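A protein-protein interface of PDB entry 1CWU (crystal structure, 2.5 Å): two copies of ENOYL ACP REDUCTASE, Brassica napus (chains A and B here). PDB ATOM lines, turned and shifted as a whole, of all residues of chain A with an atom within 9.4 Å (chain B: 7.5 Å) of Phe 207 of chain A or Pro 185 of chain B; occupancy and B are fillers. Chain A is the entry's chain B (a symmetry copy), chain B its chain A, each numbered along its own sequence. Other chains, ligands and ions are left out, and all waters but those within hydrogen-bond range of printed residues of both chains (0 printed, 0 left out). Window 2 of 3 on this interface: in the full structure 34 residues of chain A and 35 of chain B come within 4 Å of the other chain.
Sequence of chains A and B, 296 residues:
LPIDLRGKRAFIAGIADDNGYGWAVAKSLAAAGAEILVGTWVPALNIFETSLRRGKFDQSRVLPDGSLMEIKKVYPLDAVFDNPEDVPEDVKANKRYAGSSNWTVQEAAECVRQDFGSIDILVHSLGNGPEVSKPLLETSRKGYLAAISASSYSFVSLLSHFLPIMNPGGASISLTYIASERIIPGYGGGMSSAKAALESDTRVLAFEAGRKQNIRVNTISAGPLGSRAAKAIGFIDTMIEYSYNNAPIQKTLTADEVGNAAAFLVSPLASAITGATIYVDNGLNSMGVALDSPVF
The side-chain carboxylate of Glu 208 of chain A lies within hydrogen-bond range of the backbone NH of Leu 137 of chain B, at 2.7 Å.
Ala 179 of chain B touches Ser 200 of chain A (O to OG, 3.6 Å).
Arg 203 of chain A touches Ile 183 of chain B (O to CD1, 3.0 Å).
Leu 205 of chain A touches Leu 137 of chain B (CD2 to CD2, 3.5 Å).
CB of Phe 207 of chain A touches CG2 of Ile 183 of chain B, at 3.5 Å.
Pro 185 of chain B touches Phe 207 of chain A.
Of chain B, only Ile 183 and Pro 185 come within 4 Å of Phe 207 of chain A.
Of chain A, only Phe 207 comes within 4 Å of Pro 185 of chain B.
No residue of chain B comes within 4 Å of Ala 206 of chain A.
No residue of chain A comes within 4 Å of Ile 184 of chain B.
Printed residues of chain A within 4 Å of Ile 183 of chain B: Arg 203 (3.0 Å) and Phe 207 (3.5 Å).
Of the printed residues of chain A, Ala 179 of chain B touches Ser 200.
Of the printed residues of chain B, Leu 205 of chain A touches Leu 137 (3.5 Å).
Arg 182 of chain B touches none of the printed residues of chain A.
The nearest printed residue of chain B that does not touch Phe 207 of chain A is Gly 186 of chain B (6.0 Å).
The nearest residue of chain A that does not touch Pro 185 of chain B is Val 204 of chain A (6.9 Å).
The nearest printed residue of chain B that does not touch Leu 205 of chain A is Ile 183 of chain B (6.1 Å).
Of the 24 printed residues of chain A, 5 touch a printed residue of chain B.
Hydrophobic or aromatic side chains of chain A that line the printed part of chain B: Leu 205 and Phe 207.
Of the 12 printed residues of chain B, 4 touch a printed residue of chain A.
Among the printed residues, 6 pairs touch across the chains.
Among the printed residues, no Asp or Glu carboxylate lies within 4 Å of a Lys or Arg side-chain nitrogen of the other chain.
No position is printed for both chains.
Of the 6 pairs that touch across the chains among the printed residues, none has its exchanged pair printed and touching as well.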
ATOM      1  N   LEU A 159      10.112 -15.754  38.094  1.00  0.00           N
ATOM      2  CA  LEU A 159      10.390 -15.068  36.860  1.00  0.00           C
ATOM      3  C   LEU A 159       9.148 -14.430  36.274  1.00  0.00           C
ATOM      4  O   LEU A 159       9.129 -13.244  35.944  1.00  0.00           O
ATOM      5  CB  LEU A 159      11.015 -16.021  35.853  1.00  0.00           C
ATOM      6  CG  LEU A 159      11.425 -15.319  34.560  1.00  0.00           C
ATOM      7  CD1 LEU A 159      12.476 -14.244  34.837  1.00  0.00           C
ATOM      8  CD2 LEU A 159      11.918 -16.327  33.542  1.00  0.00           C
ATOM      9  N   LEU A 163       9.305 -10.580  36.236  1.00  0.00           N
ATOM     10  CA  LEU A 163       9.581 -10.178  34.845  1.00  0.00           C
ATOM     11  C   LEU A 163       8.943  -8.875  34.444  1.00  0.00           C
ATOM     12  O   LEU A 163       9.447  -8.199  33.566  1.00  0.00           O
ATOM     13  CB  LEU A 163       9.114 -11.255  33.855  1.00  0.00           C
ATOM     14  CG  LEU A 163       9.703 -11.115  32.464  1.00  0.00           C
ATOM     15  CD1 LEU A 163      11.107 -11.655  32.502  1.00  0.00           C
ATOM     16  CD2 LEU A 163       8.877 -11.720  31.353  1.00  0.00           C
ATOM     17  N   SER A 200      15.084 -27.633  31.725  1.00  0.00           N
ATOM     18  CA  SER A 200      14.312 -27.460  30.515  1.00  0.00           C
ATOM     19  C   SER A 200      13.667 -26.089  30.435  1.00  0.00           C
ATOM     20  O   SER A 200      13.708 -25.441  29.400  1.00  0.00           O
ATOM     21  CB  SER A 200      13.288 -28.572  30.332  1.00  0.00           C
ATOM     22  OG  SER A 200      12.557 -28.358  29.132  1.00  0.00           O
ATOM     23  N   ASP A 201      13.094 -25.622  31.538  1.00  0.00           N
ATOM     24  CA  ASP A 201      12.438 -24.304  31.535  1.00  0.00           C
ATOM     25  C   ASP A 201      13.379 -23.124  31.359  1.00  0.00           C
ATOM     26  O   ASP A 201      12.940 -22.043  30.955  1.00  0.00           O
ATOM     27  CB  ASP A 201      11.595 -24.088  32.785  1.00  0.00           C
ATOM     28  CG  ASP A 201      10.508 -25.112  32.940  1.00  0.00           C
ATOM     29  OD1 ASP A 201       9.954 -25.572  31.909  1.00  0.00           O
ATOM     30  OD2 ASP A 201      10.156 -25.378  34.110  1.00  0.00           O
ATOM     31  N   THR A 202      14.655 -23.300  31.694  1.00  0.00           N
ATOM     32  CA  THR A 202      15.582 -22.194  31.534  1.00  0.00           C
ATOM     33  C   THR A 202      15.596 -21.859  30.073  1.00  0.00           C
ATOM     34  O   THR A 202      15.454 -20.706  29.664  1.00  0.00           O
ATOM     35  CB  THR A 202      16.990 -22.590  31.899  1.00  0.00           C
ATOM     36  OG1 THR A 202      16.996 -23.151  33.211  1.00  0.00           O
ATOM     37  CG2 THR A 202      17.900 -21.386  31.832  1.00  0.00           C
ATOM     38  N   ARG A 203      15.737 -22.902  29.270  1.00  0.00           N
ATOM     39  CA  ARG A 203      15.777 -22.732  27.842  1.00  0.00           C
ATOM     40  C   ARG A 203      14.504 -22.105  27.361  1.00  0.00           C
ATOM     41  O   ARG A 203      14.527 -21.123  26.627  1.00  0.00           O
ATOM     42  CB  ARG A 203      15.956 -24.083  27.154  1.00  0.00           C
ATOM     43  CG  ARG A 203      17.226 -24.765  27.520  1.00  0.00           C
ATOM     44  CD  ARG A 203      17.379 -26.021  26.693  1.00  0.00           C
ATOM     45  NE  ARG A 203      16.822 -27.192  27.364  1.00  0.00           N
ATOM     46  CZ  ARG A 203      17.432 -27.824  28.367  1.00  0.00           C
ATOM     47  NH1 ARG A 203      18.595 -27.400  28.831  1.00  0.00           N
ATOM     48  NH2 ARG A 203      16.870 -28.874  28.934  1.00  0.00           N
ATOM     49  N   VAL A 204      13.374 -22.697  27.726  1.00  0.00           N
ATOM     50  CA  VAL A 204      12.115 -22.169  27.224  1.00  0.00           C
ATOM     51  C   VAL A 204      11.813 -20.755  27.656  1.00  0.00           C
ATOM     52  O   VAL A 204      11.260 -19.949  26.869  1.00  0.00           O
ATOM     53  CB  VAL A 204      10.919 -23.075  27.504  1.00  0.00           C
ATOM     54  CG1 VAL A 204       9.672 -22.393  27.012  1.00  0.00           C
ATOM     55  CG2 VAL A 204      11.086 -24.425  26.809  1.00  0.00           C
ATOM     56  N   LEU A 205      12.169 -20.443  28.905  1.00  0.00           N
ATOM     57  CA  LEU A 205      11.968 -19.094  29.437  1.00  0.00           C
ATOM     58  C   LEU A 205      12.931 -18.067  28.804  1.00  0.00           C
ATOM     59  O   LEU A 205      12.552 -16.911  28.570  1.00  0.00           O
ATOM     60  CB  LEU A 205      12.004 -19.115  30.958  1.00  0.00           C
ATOM     61  CG  LEU A 205      10.676 -19.672  31.499  1.00  0.00           C
ATOM     62  CD1 LEU A 205      10.799 -20.063  32.947  1.00  0.00           C
ATOM     63  CD2 LEU A 205       9.588 -18.626  31.287  1.00  0.00           C
ATOM     64  N   ALA A 206      14.129 -18.529  28.421  1.00  0.00           N
ATOM     65  CA  ALA A 206      15.093 -17.683  27.699  1.00  0.00           C
ATOM     66  C   ALA A 206      14.445 -17.278  26.403  1.00  0.00           C
ATOM     67  O   ALA A 206      14.575 -16.147  25.935  1.00  0.00           O
ATOM     68  CB  ALA A 206      16.400 -18.442  27.429  1.00  0.00           C
ATOM     69  N   PHE A 207      13.719 -18.204  25.807  1.00  0.00           N
ATOM     70  CA  PHE A 207      13.024 -17.848  24.615  1.00  0.00           C
ATOM     71  C   PHE A 207      11.907 -16.875  24.999  1.00  0.00           C
ATOM     72  O   PHE A 207      11.861 -15.743  24.537  1.00  0.00           O
ATOM     73  CB  PHE A 207      12.469 -19.080  23.930  1.00  0.00           C
ATOM     74  CG  PHE A 207      11.509 -18.758  22.826  1.00  0.00           C
ATOM     75  CD1 PHE A 207      11.936 -18.063  21.711  1.00  0.00           C
ATOM     76  CD2 PHE A 207      10.191 -19.172  22.892  1.00  0.00           C
ATOM     77  CE1 PHE A 207      11.060 -17.760  20.673  1.00  0.00           C
ATOM     78  CE2 PHE A 207       9.329 -18.889  21.868  1.00  0.00           C
ATOM     79  CZ  PHE A 207       9.757 -18.155  20.767  1.00  0.00           C
ATOM     80  N   GLU A 208      11.033 -17.297  25.896  1.00  0.00           N
ATOM     81  CA  GLU A 208       9.904 -16.451  26.288  1.00  0.00           C
ATOM     82  C   GLU A 208      10.276 -15.074  26.783  1.00  0.00           C
ATOM     83  O   GLU A 208       9.840 -14.076  26.215  1.00  0.00           O
ATOM     84  CB  GLU A 208       9.017 -17.166  27.299  1.00  0.00           C
ATOM     85  CG  GLU A 208       8.049 -18.150  26.664  1.00  0.00           C
ATOM     86  CD  GLU A 208       7.394 -19.064  27.659  1.00  0.00           C
ATOM     87  OE1 GLU A 208       7.279 -18.702  28.846  1.00  0.00           O
ATOM     88  OE2 GLU A 208       7.050 -20.179  27.262  1.00  0.00           O
ATOM     89  N   ALA A 209      11.051 -15.005  27.868  1.00  0.00           N
ATOM     90  CA  ALA A 209      11.457 -13.706  28.410  1.00  0.00           C
ATOM     91  C   ALA A 209      12.423 -13.016  27.462  1.00  0.00           C
ATOM     92  O   ALA A 209      12.421 -11.795  27.321  1.00  0.00           O
ATOM     93  CB  ALA A 209      12.056 -13.846  29.811  1.00  0.00           C
ATOM     94  N   GLY A 210      13.213 -13.806  26.757  1.00  0.00           N
ATOM     95  CA  GLY A 210      14.163 -13.252  25.822  1.00  0.00           C
ATOM     96  C   GLY A 210      13.439 -12.436  24.767  1.00  0.00           C
ATOM     97  O   GLY A 210      13.851 -11.337  24.392  1.00  0.00           O
ATOM     98  N   ARG A 211      12.373 -12.996  24.247  1.00  0.00           N
ATOM     99  CA  ARG A 211      11.674 -12.334  23.178  1.00  0.00           C
ATOM    100  C   ARG A 211      10.707 -11.295  23.644  1.00  0.00           C
ATOM    101  O   ARG A 211      10.334 -10.389  22.883  1.00  0.00           O
ATOM    102  CB  ARG A 211      10.974 -13.367  22.332  1.00  0.00           C
ATOM    103  CG  ARG A 211      11.930 -14.200  21.511  1.00  0.00           C
ATOM    104  CD  ARG A 211      12.748 -13.325  20.589  1.00  0.00           C
ATOM    105  NE  ARG A 211      13.604 -14.122  19.729  1.00  0.00           N
ATOM    106  CZ  ARG A 211      13.526 -14.133  18.415  1.00  0.00           C
ATOM    107  NH1 ARG A 211      12.631 -13.364  17.814  1.00  0.00           N
ATOM    108  NH2 ARG A 211      14.369 -14.882  17.710  1.00  0.00           N
ATOM    109  N   LYS A 212      10.271 -11.435  24.891  1.00  0.00           N
ATOM    110  CA  LYS A 212       9.293 -10.513  25.455  1.00  0.00           C
ATOM    111  C   LYS A 212       9.832  -9.260  26.137  1.00  0.00           C
ATOM    112  O   LYS A 212       9.207  -8.207  26.075  1.00  0.00           O
ATOM    113  CB  LYS A 212       8.367 -11.240  26.414  1.00  0.00           C
ATOM    114  CG  LYS A 212       7.488 -10.294  27.191  1.00  0.00           C
ATOM    115  CD  LYS A 212       6.292 -11.009  27.721  1.00  0.00           C
ATOM    116  CE  LYS A 212       5.376 -10.064  28.424  1.00  0.00           C
ATOM    117  NZ  LYS A 212       4.310 -10.844  29.116  1.00  0.00           N
ATOM    118  N   GLN A 213      10.976  -9.379  26.800  1.00  0.00           N
ATOM    119  CA  GLN A 213      11.533  -8.275  27.586  1.00  0.00           C
ATOM    120  C   GLN A 213      13.055  -8.225  27.464  1.00  0.00           C
ATOM    121  O   GLN A 213      13.733  -7.641  28.289  1.00  0.00           O
ATOM    122  CB  GLN A 213      11.183  -8.540  29.057  1.00  0.00           C
ATOM    123  CG  GLN A 213      11.331  -7.373  29.961  1.00  0.00           C
ATOM    124  CD  GLN A 213      10.151  -6.451  29.873  1.00  0.00           C
ATOM    125  OE1 GLN A 213       9.452  -6.424  28.850  1.00  0.00           O
ATOM    126  NE2 GLN A 213       9.809  -5.820  30.998  1.00  0.00           N
ATOM    127  N   ASN A 214      13.598  -8.952  26.507  1.00  0.00           N
ATOM    128  CA  ASN A 214      15.043  -8.990  26.326  1.00  0.00           C
ATOM    129  C   ASN A 214      15.800  -9.315  27.577  1.00  0.00           C
ATOM    130  O   ASN A 214      16.864  -8.768  27.833  1.00  0.00           O
ATOM    131  CB  ASN A 214      15.555  -7.704  25.700  1.00  0.00           C
ATOM    132  CG  ASN A 214      15.159  -7.583  24.255  1.00  0.00           C
ATOM    133  OD1 ASN A 214      16.003  -7.689  23.357  1.00  0.00           O
ATOM    134  ND2 ASN A 214      13.861  -7.422  24.007  1.00  0.00           N
ATOM    135  N   ILE A 215      15.243 -10.228  28.349  1.00  0.00           N
ATOM    136  CA  ILE A 215      15.852 -10.682  29.584  1.00  0.00           C
ATOM    137  C   ILE A 215      16.578 -11.987  29.283  1.00  0.00           C
ATOM    138  O   ILE A 215      16.127 -12.755  28.447  1.00  0.00           O
ATOM    139  CB  ILE A 215      14.704 -10.924  30.632  1.00  0.00           C
ATOM    140  CG1 ILE A 215      14.016  -9.593  30.983  1.00  0.00           C
ATOM    141  CG2 ILE A 215      15.190 -11.709  31.871  1.00  0.00           C
ATOM    142  CD1 ILE A 215      14.961  -8.549  31.584  1.00  0.00           C
ATOM    143  N   ARG A 216      17.698 -12.252  29.946  1.00  0.00           N
ATOM    144  CA  ARG A 216      18.407 -13.506  29.709  1.00  0.00           C
ATOM    145  C   ARG A 216      18.109 -14.474  30.826  1.00  0.00           C
ATOM    146  O   ARG A 216      17.827 -14.055  31.944  1.00  0.00           O
ATOM    147  CB  ARG A 216      19.914 -13.299  29.553  1.00  0.00           C
ATOM    148  CG  ARG A 216      20.304 -12.634  28.243  1.00  0.00           C
ATOM    149  CD  ARG A 216      21.822 -12.598  28.085  1.00  0.00           C
ATOM    150  NE  ARG A 216      22.439 -11.747  29.102  1.00  0.00           N
ATOM    151  CZ  ARG A 216      22.987 -12.195  30.228  1.00  0.00           C
ATOM    152  NH1 ARG A 216      23.019 -13.492  30.478  1.00  0.00           N
ATOM    153  NH2 ARG A 216      23.510 -11.341  31.107  1.00  0.00           N
ATOM    154  N   VAL A 217      18.213 -15.767  30.540  1.00  0.00           N
ATOM    155  CA  VAL A 217      17.903 -16.777  31.536  1.00  0.00           C
ATOM    156  C   VAL A 217      18.884 -17.907  31.421  1.00  0.00           C
ATOM    157  O   VAL A 217      18.975 -18.543  30.385  1.00  0.00           O
ATOM    158  CB  VAL A 217      16.475 -17.399  31.299  1.00  0.00           C
ATOM    159  CG1 VAL A 217      16.246 -18.544  32.217  1.00  0.00           C
ATOM    160  CG2 VAL A 217      15.401 -16.385  31.502  1.00  0.00           C
ATOM    161  N   ASN A 218      19.562 -18.202  32.511  1.00  0.00           N
ATOM    162  CA  ASN A 218      20.520 -19.279  32.524  1.00  0.00           C
ATOM    163  C   ASN A 218      20.431 -19.998  33.839  1.00  0.00           C
ATOM    164  O   ASN A 218      19.735 -19.532  34.739  1.00  0.00           O
ATOM    165  CB  ASN A 218      21.930 -18.724  32.320  1.00  0.00           C
ATOM    166  CG  ASN A 218      22.117 -18.124  30.927  1.00  0.00           C
ATOM    167  OD1 ASN A 218      21.888 -18.795  29.919  1.00  0.00           O
ATOM    168  ND2 ASN A 218      22.413 -16.832  30.872  1.00  0.00           N
ATOM    169  N   THR A 274      22.533 -17.015  26.823  1.00  0.00           N
ATOM    170  CA  THR A 274      21.180 -17.224  27.358  1.00  0.00           C
ATOM    171  C   THR A 274      20.666 -18.647  27.120  1.00  0.00           C
ATOM    172  O   THR A 274      21.051 -19.305  26.144  1.00  0.00           O
ATOM    173  CB  THR A 274      20.172 -16.165  26.890  1.00  0.00           C
ATOM    174  OG1 THR A 274      19.014 -16.234  27.713  1.00  0.00           O
ATOM    175  CG2 THR A 274      19.757 -16.383  25.502  1.00  0.00           C
ATOM    176  N   GLY A 275      19.821 -19.138  28.030  1.00  0.00           N
ATOM    177  CA  GLY A 275      19.248 -20.496  27.922  1.00  0.00           C
ATOM    178  C   GLY A 275      20.301 -21.588  28.182  1.00  0.00           C
ATOM    179  O   GLY A 275      20.158 -22.737  27.755  1.00  0.00           O
ATOM    180  N   ALA A 276      21.382 -21.216  28.854  1.00  0.00           N
ATOM    181  CA  ALA A 276      22.466 -22.149  29.130  1.00  0.00           C
ATOM    182  C   ALA A 276      22.430 -22.859  30.468  1.00  0.00           C
ATOM    183  O   ALA A 276      21.821 -22.410  31.447  1.00  0.00           O
ATOM    184  CB  ALA A 276      23.807 -21.459  28.951  1.00  0.00           C
ATOM    185  N   LEU B 137       5.365 -18.826  30.707  1.00  0.00           N
ATOM    186  CA  LEU B 137       5.087 -17.561  31.413  1.00  0.00           C
ATOM    187  C   LEU B 137       3.623 -17.412  31.803  1.00  0.00           C
ATOM    188  O   LEU B 137       3.316 -16.989  32.900  1.00  0.00           O
ATOM    189  CB  LEU B 137       5.500 -16.351  30.579  1.00  0.00           C
ATOM    190  CG  LEU B 137       6.992 -16.079  30.382  1.00  0.00           C
ATOM    191  CD1 LEU B 137       7.121 -14.960  29.390  1.00  0.00           C
ATOM    192  CD2 LEU B 137       7.682 -15.724  31.687  1.00  0.00           C
ATOM    193  N   TYR B 177       9.432 -36.217  23.769  1.00  0.00           N
ATOM    194  CA  TYR B 177       9.449 -35.263  22.659  1.00  0.00           C
ATOM    195  C   TYR B 177      10.600 -34.270  22.847  1.00  0.00           C
ATOM    196  O   TYR B 177      11.040 -34.039  23.973  1.00  0.00           O
ATOM    197  CB  TYR B 177       8.077 -34.578  22.485  1.00  0.00           C
ATOM    198  CG  TYR B 177       8.020 -33.560  21.353  1.00  0.00           C
ATOM    199  CD1 TYR B 177       8.360 -33.919  20.049  1.00  0.00           C
ATOM    200  CD2 TYR B 177       7.593 -32.269  21.573  1.00  0.00           C
ATOM    201  CE1 TYR B 177       8.323 -33.008  19.018  1.00  0.00           C
ATOM    202  CE2 TYR B 177       7.557 -31.335  20.534  1.00  0.00           C
ATOM    203  CZ  TYR B 177       7.943 -31.715  19.275  1.00  0.00           C
ATOM    204  OH  TYR B 177       7.951 -30.811  18.262  1.00  0.00           O
ATOM    205  N   ALA B 179      10.981 -31.124  22.843  1.00  0.00           N
ATOM    206  CA  ALA B 179      10.717 -29.944  23.681  1.00  0.00           C
ATOM    207  C   ALA B 179      11.331 -30.040  25.057  1.00  0.00           C
ATOM    208  O   ALA B 179      11.629 -29.034  25.671  1.00  0.00           O
ATOM    209  CB  ALA B 179       9.238 -29.663  23.794  1.00  0.00           C
ATOM    210  N   ARG B 182      14.983 -28.989  23.820  1.00  0.00           N
ATOM    211  CA  ARG B 182      15.221 -27.797  23.044  1.00  0.00           C
ATOM    212  C   ARG B 182      13.978 -26.978  23.048  1.00  0.00           C
ATOM    213  O   ARG B 182      12.936 -27.447  23.456  1.00  0.00           O
ATOM    214  CB  ARG B 182      15.555 -28.214  21.628  1.00  0.00           C
ATOM    215  CG  ARG B 182      16.659 -29.275  21.606  1.00  0.00           C
ATOM    216  CD  ARG B 182      17.950 -28.699  21.039  1.00  0.00           C
ATOM    217  NE  ARG B 182      17.925 -28.762  19.580  1.00  0.00           N
ATOM    218  CZ  ARG B 182      18.376 -29.808  18.888  1.00  0.00           C
ATOM    219  NH1 ARG B 182      18.948 -30.831  19.524  1.00  0.00           N
ATOM    220  NH2 ARG B 182      18.296 -29.823  17.568  1.00  0.00           N
ATOM    221  N   ILE B 183      14.094 -25.727  22.643  1.00  0.00           N
ATOM    222  CA  ILE B 183      12.960 -24.835  22.675  1.00  0.00           C
ATOM    223  C   ILE B 183      12.102 -25.088  21.475  1.00  0.00           C
ATOM    224  O   ILE B 183      12.559 -24.929  20.343  1.00  0.00           O
ATOM    225  CB  ILE B 183      13.438 -23.385  22.736  1.00  0.00           C
ATOM    226  CG1 ILE B 183      14.462 -23.261  23.851  1.00  0.00           C
ATOM    227  CG2 ILE B 183      12.275 -22.381  22.943  1.00  0.00           C
ATOM    228  CD1 ILE B 183      15.221 -21.937  23.798  1.00  0.00           C
ATOM    229  N   ILE B 184      10.852 -25.485  21.728  1.00  0.00           N
ATOM    230  CA  ILE B 184       9.868 -25.738  20.672  1.00  0.00           C
ATOM    231  C   ILE B 184       8.706 -24.819  20.938  1.00  0.00           C
ATOM    232  O   ILE B 184       7.902 -25.052  21.835  1.00  0.00           O
ATOM    233  CB  ILE B 184       9.270 -27.129  20.796  1.00  0.00           C
ATOM    234  CG1 ILE B 184      10.352 -28.203  20.700  1.00  0.00           C
ATOM    235  CG2 ILE B 184       8.171 -27.298  19.760  1.00  0.00           C
ATOM    236  CD1 ILE B 184      10.952 -28.304  19.323  1.00  0.00           C
ATOM    237  N   PRO B 185       8.638 -23.716  20.221  1.00  0.00           N
ATOM    238  CA  PRO B 185       7.544 -22.825  20.492  1.00  0.00           C
ATOM    239  C   PRO B 185       6.232 -23.598  20.324  1.00  0.00           C
ATOM    240  O   PRO B 185       6.166 -24.516  19.524  1.00  0.00           O
ATOM    241  CB  PRO B 185       7.703 -21.762  19.402  1.00  0.00           C
ATOM    242  CG  PRO B 185       9.171 -21.603  19.279  1.00  0.00           C
ATOM    243  CD  PRO B 185       9.768 -23.000  19.589  1.00  0.00           C
ATOM    244  N   GLY B 186       5.204 -23.216  21.077  1.00  0.00           N
ATOM    245  CA  GLY B 186       3.877 -23.837  20.981  1.00  0.00           C
ATOM    246  C   GLY B 186       3.543 -25.042  21.894  1.00  0.00           C
ATOM    247  O   GLY B 186       2.395 -25.371  22.086  1.00  0.00           O
ATOM    248  N   TYR B 187       4.542 -25.703  22.433  1.00  0.00           N
ATOM    249  CA  TYR B 187       4.305 -26.850  23.268  1.00  0.00           C
ATOM    250  C   TYR B 187       4.415 -26.347  24.687  1.00  0.00           C
ATOM    251  O   TYR B 187       5.418 -26.552  25.351  1.00  0.00           O
ATOM    252  CB  TYR B 187       5.398 -27.885  22.973  1.00  0.00           C
ATOM    253  CG  TYR B 187       5.196 -29.272  23.555  1.00  0.00           C
ATOM    254  CD1 TYR B 187       4.309 -30.156  22.979  1.00  0.00           C
ATOM    255  CD2 TYR B 187       6.000 -29.737  24.585  1.00  0.00           C
ATOM    256  CE1 TYR B 187       4.177 -31.444  23.465  1.00  0.00           C
ATOM    257  CE2 TYR B 187       5.864 -31.020  25.087  1.00  0.00           C
ATOM    258  CZ  TYR B 187       4.964 -31.879  24.507  1.00  0.00           C
ATOM    259  OH  TYR B 187       4.825 -33.172  24.985  1.00  0.00           O
ATOM    260  N   GLY B 188       3.375 -25.699  25.177  1.00  0.00           N
ATOM    261  CA  GLY B 188       3.460 -25.144  26.521  1.00  0.00           C
ATOM    262  C   GLY B 188       2.900 -25.926  27.684  1.00  0.00           C
ATOM    263  O   GLY B 188       3.070 -27.163  27.822  1.00  0.00           O
ATOM    264  N   PHE B 235      -0.554 -27.631  16.687  1.00  0.00           N
ATOM    265  CA  PHE B 235       0.607 -27.176  15.945  1.00  0.00           C
ATOM    266  C   PHE B 235       1.249 -28.287  15.146  1.00  0.00           C
ATOM    267  O   PHE B 235       2.177 -28.066  14.359  1.00  0.00           O
ATOM    268  CB  PHE B 235       1.604 -26.511  16.897  1.00  0.00           C
ATOM    269  CG  PHE B 235       2.351 -27.466  17.774  1.00  0.00           C
ATOM    270  CD1 PHE B 235       3.553 -27.095  18.346  1.00  0.00           C
ATOM    271  CD2 PHE B 235       1.893 -28.755  17.978  1.00  0.00           C
ATOM    272  CE1 PHE B 235       4.265 -27.975  19.132  1.00  0.00           C
ATOM    273  CE2 PHE B 235       2.603 -29.646  18.780  1.00  0.00           C
ATOM    274  CZ  PHE B 235       3.791 -29.258  19.334  1.00  0.00           C
ATOM    275  N   MET B 239       4.273 -28.701  12.291  1.00  0.00           N
ATOM    276  CA  MET B 239       5.423 -29.448  12.740  1.00  0.00           C
ATOM    277  C   MET B 239       5.777 -30.597  11.784  1.00  0.00           C
ATOM    278  O   MET B 239       6.950 -30.954  11.593  1.00  0.00           O
ATOM    279  CB  MET B 239       5.183 -29.948  14.158  1.00  0.00           C
ATOM    280  CG  MET B 239       5.137 -28.812  15.181  1.00  0.00           C
ATOM    281  SD  MET B 239       6.634 -27.735  15.162  1.00  0.00           S
ATOM    282  CE  MET B 239       8.032 -28.978  15.265  1.00  0.00           C
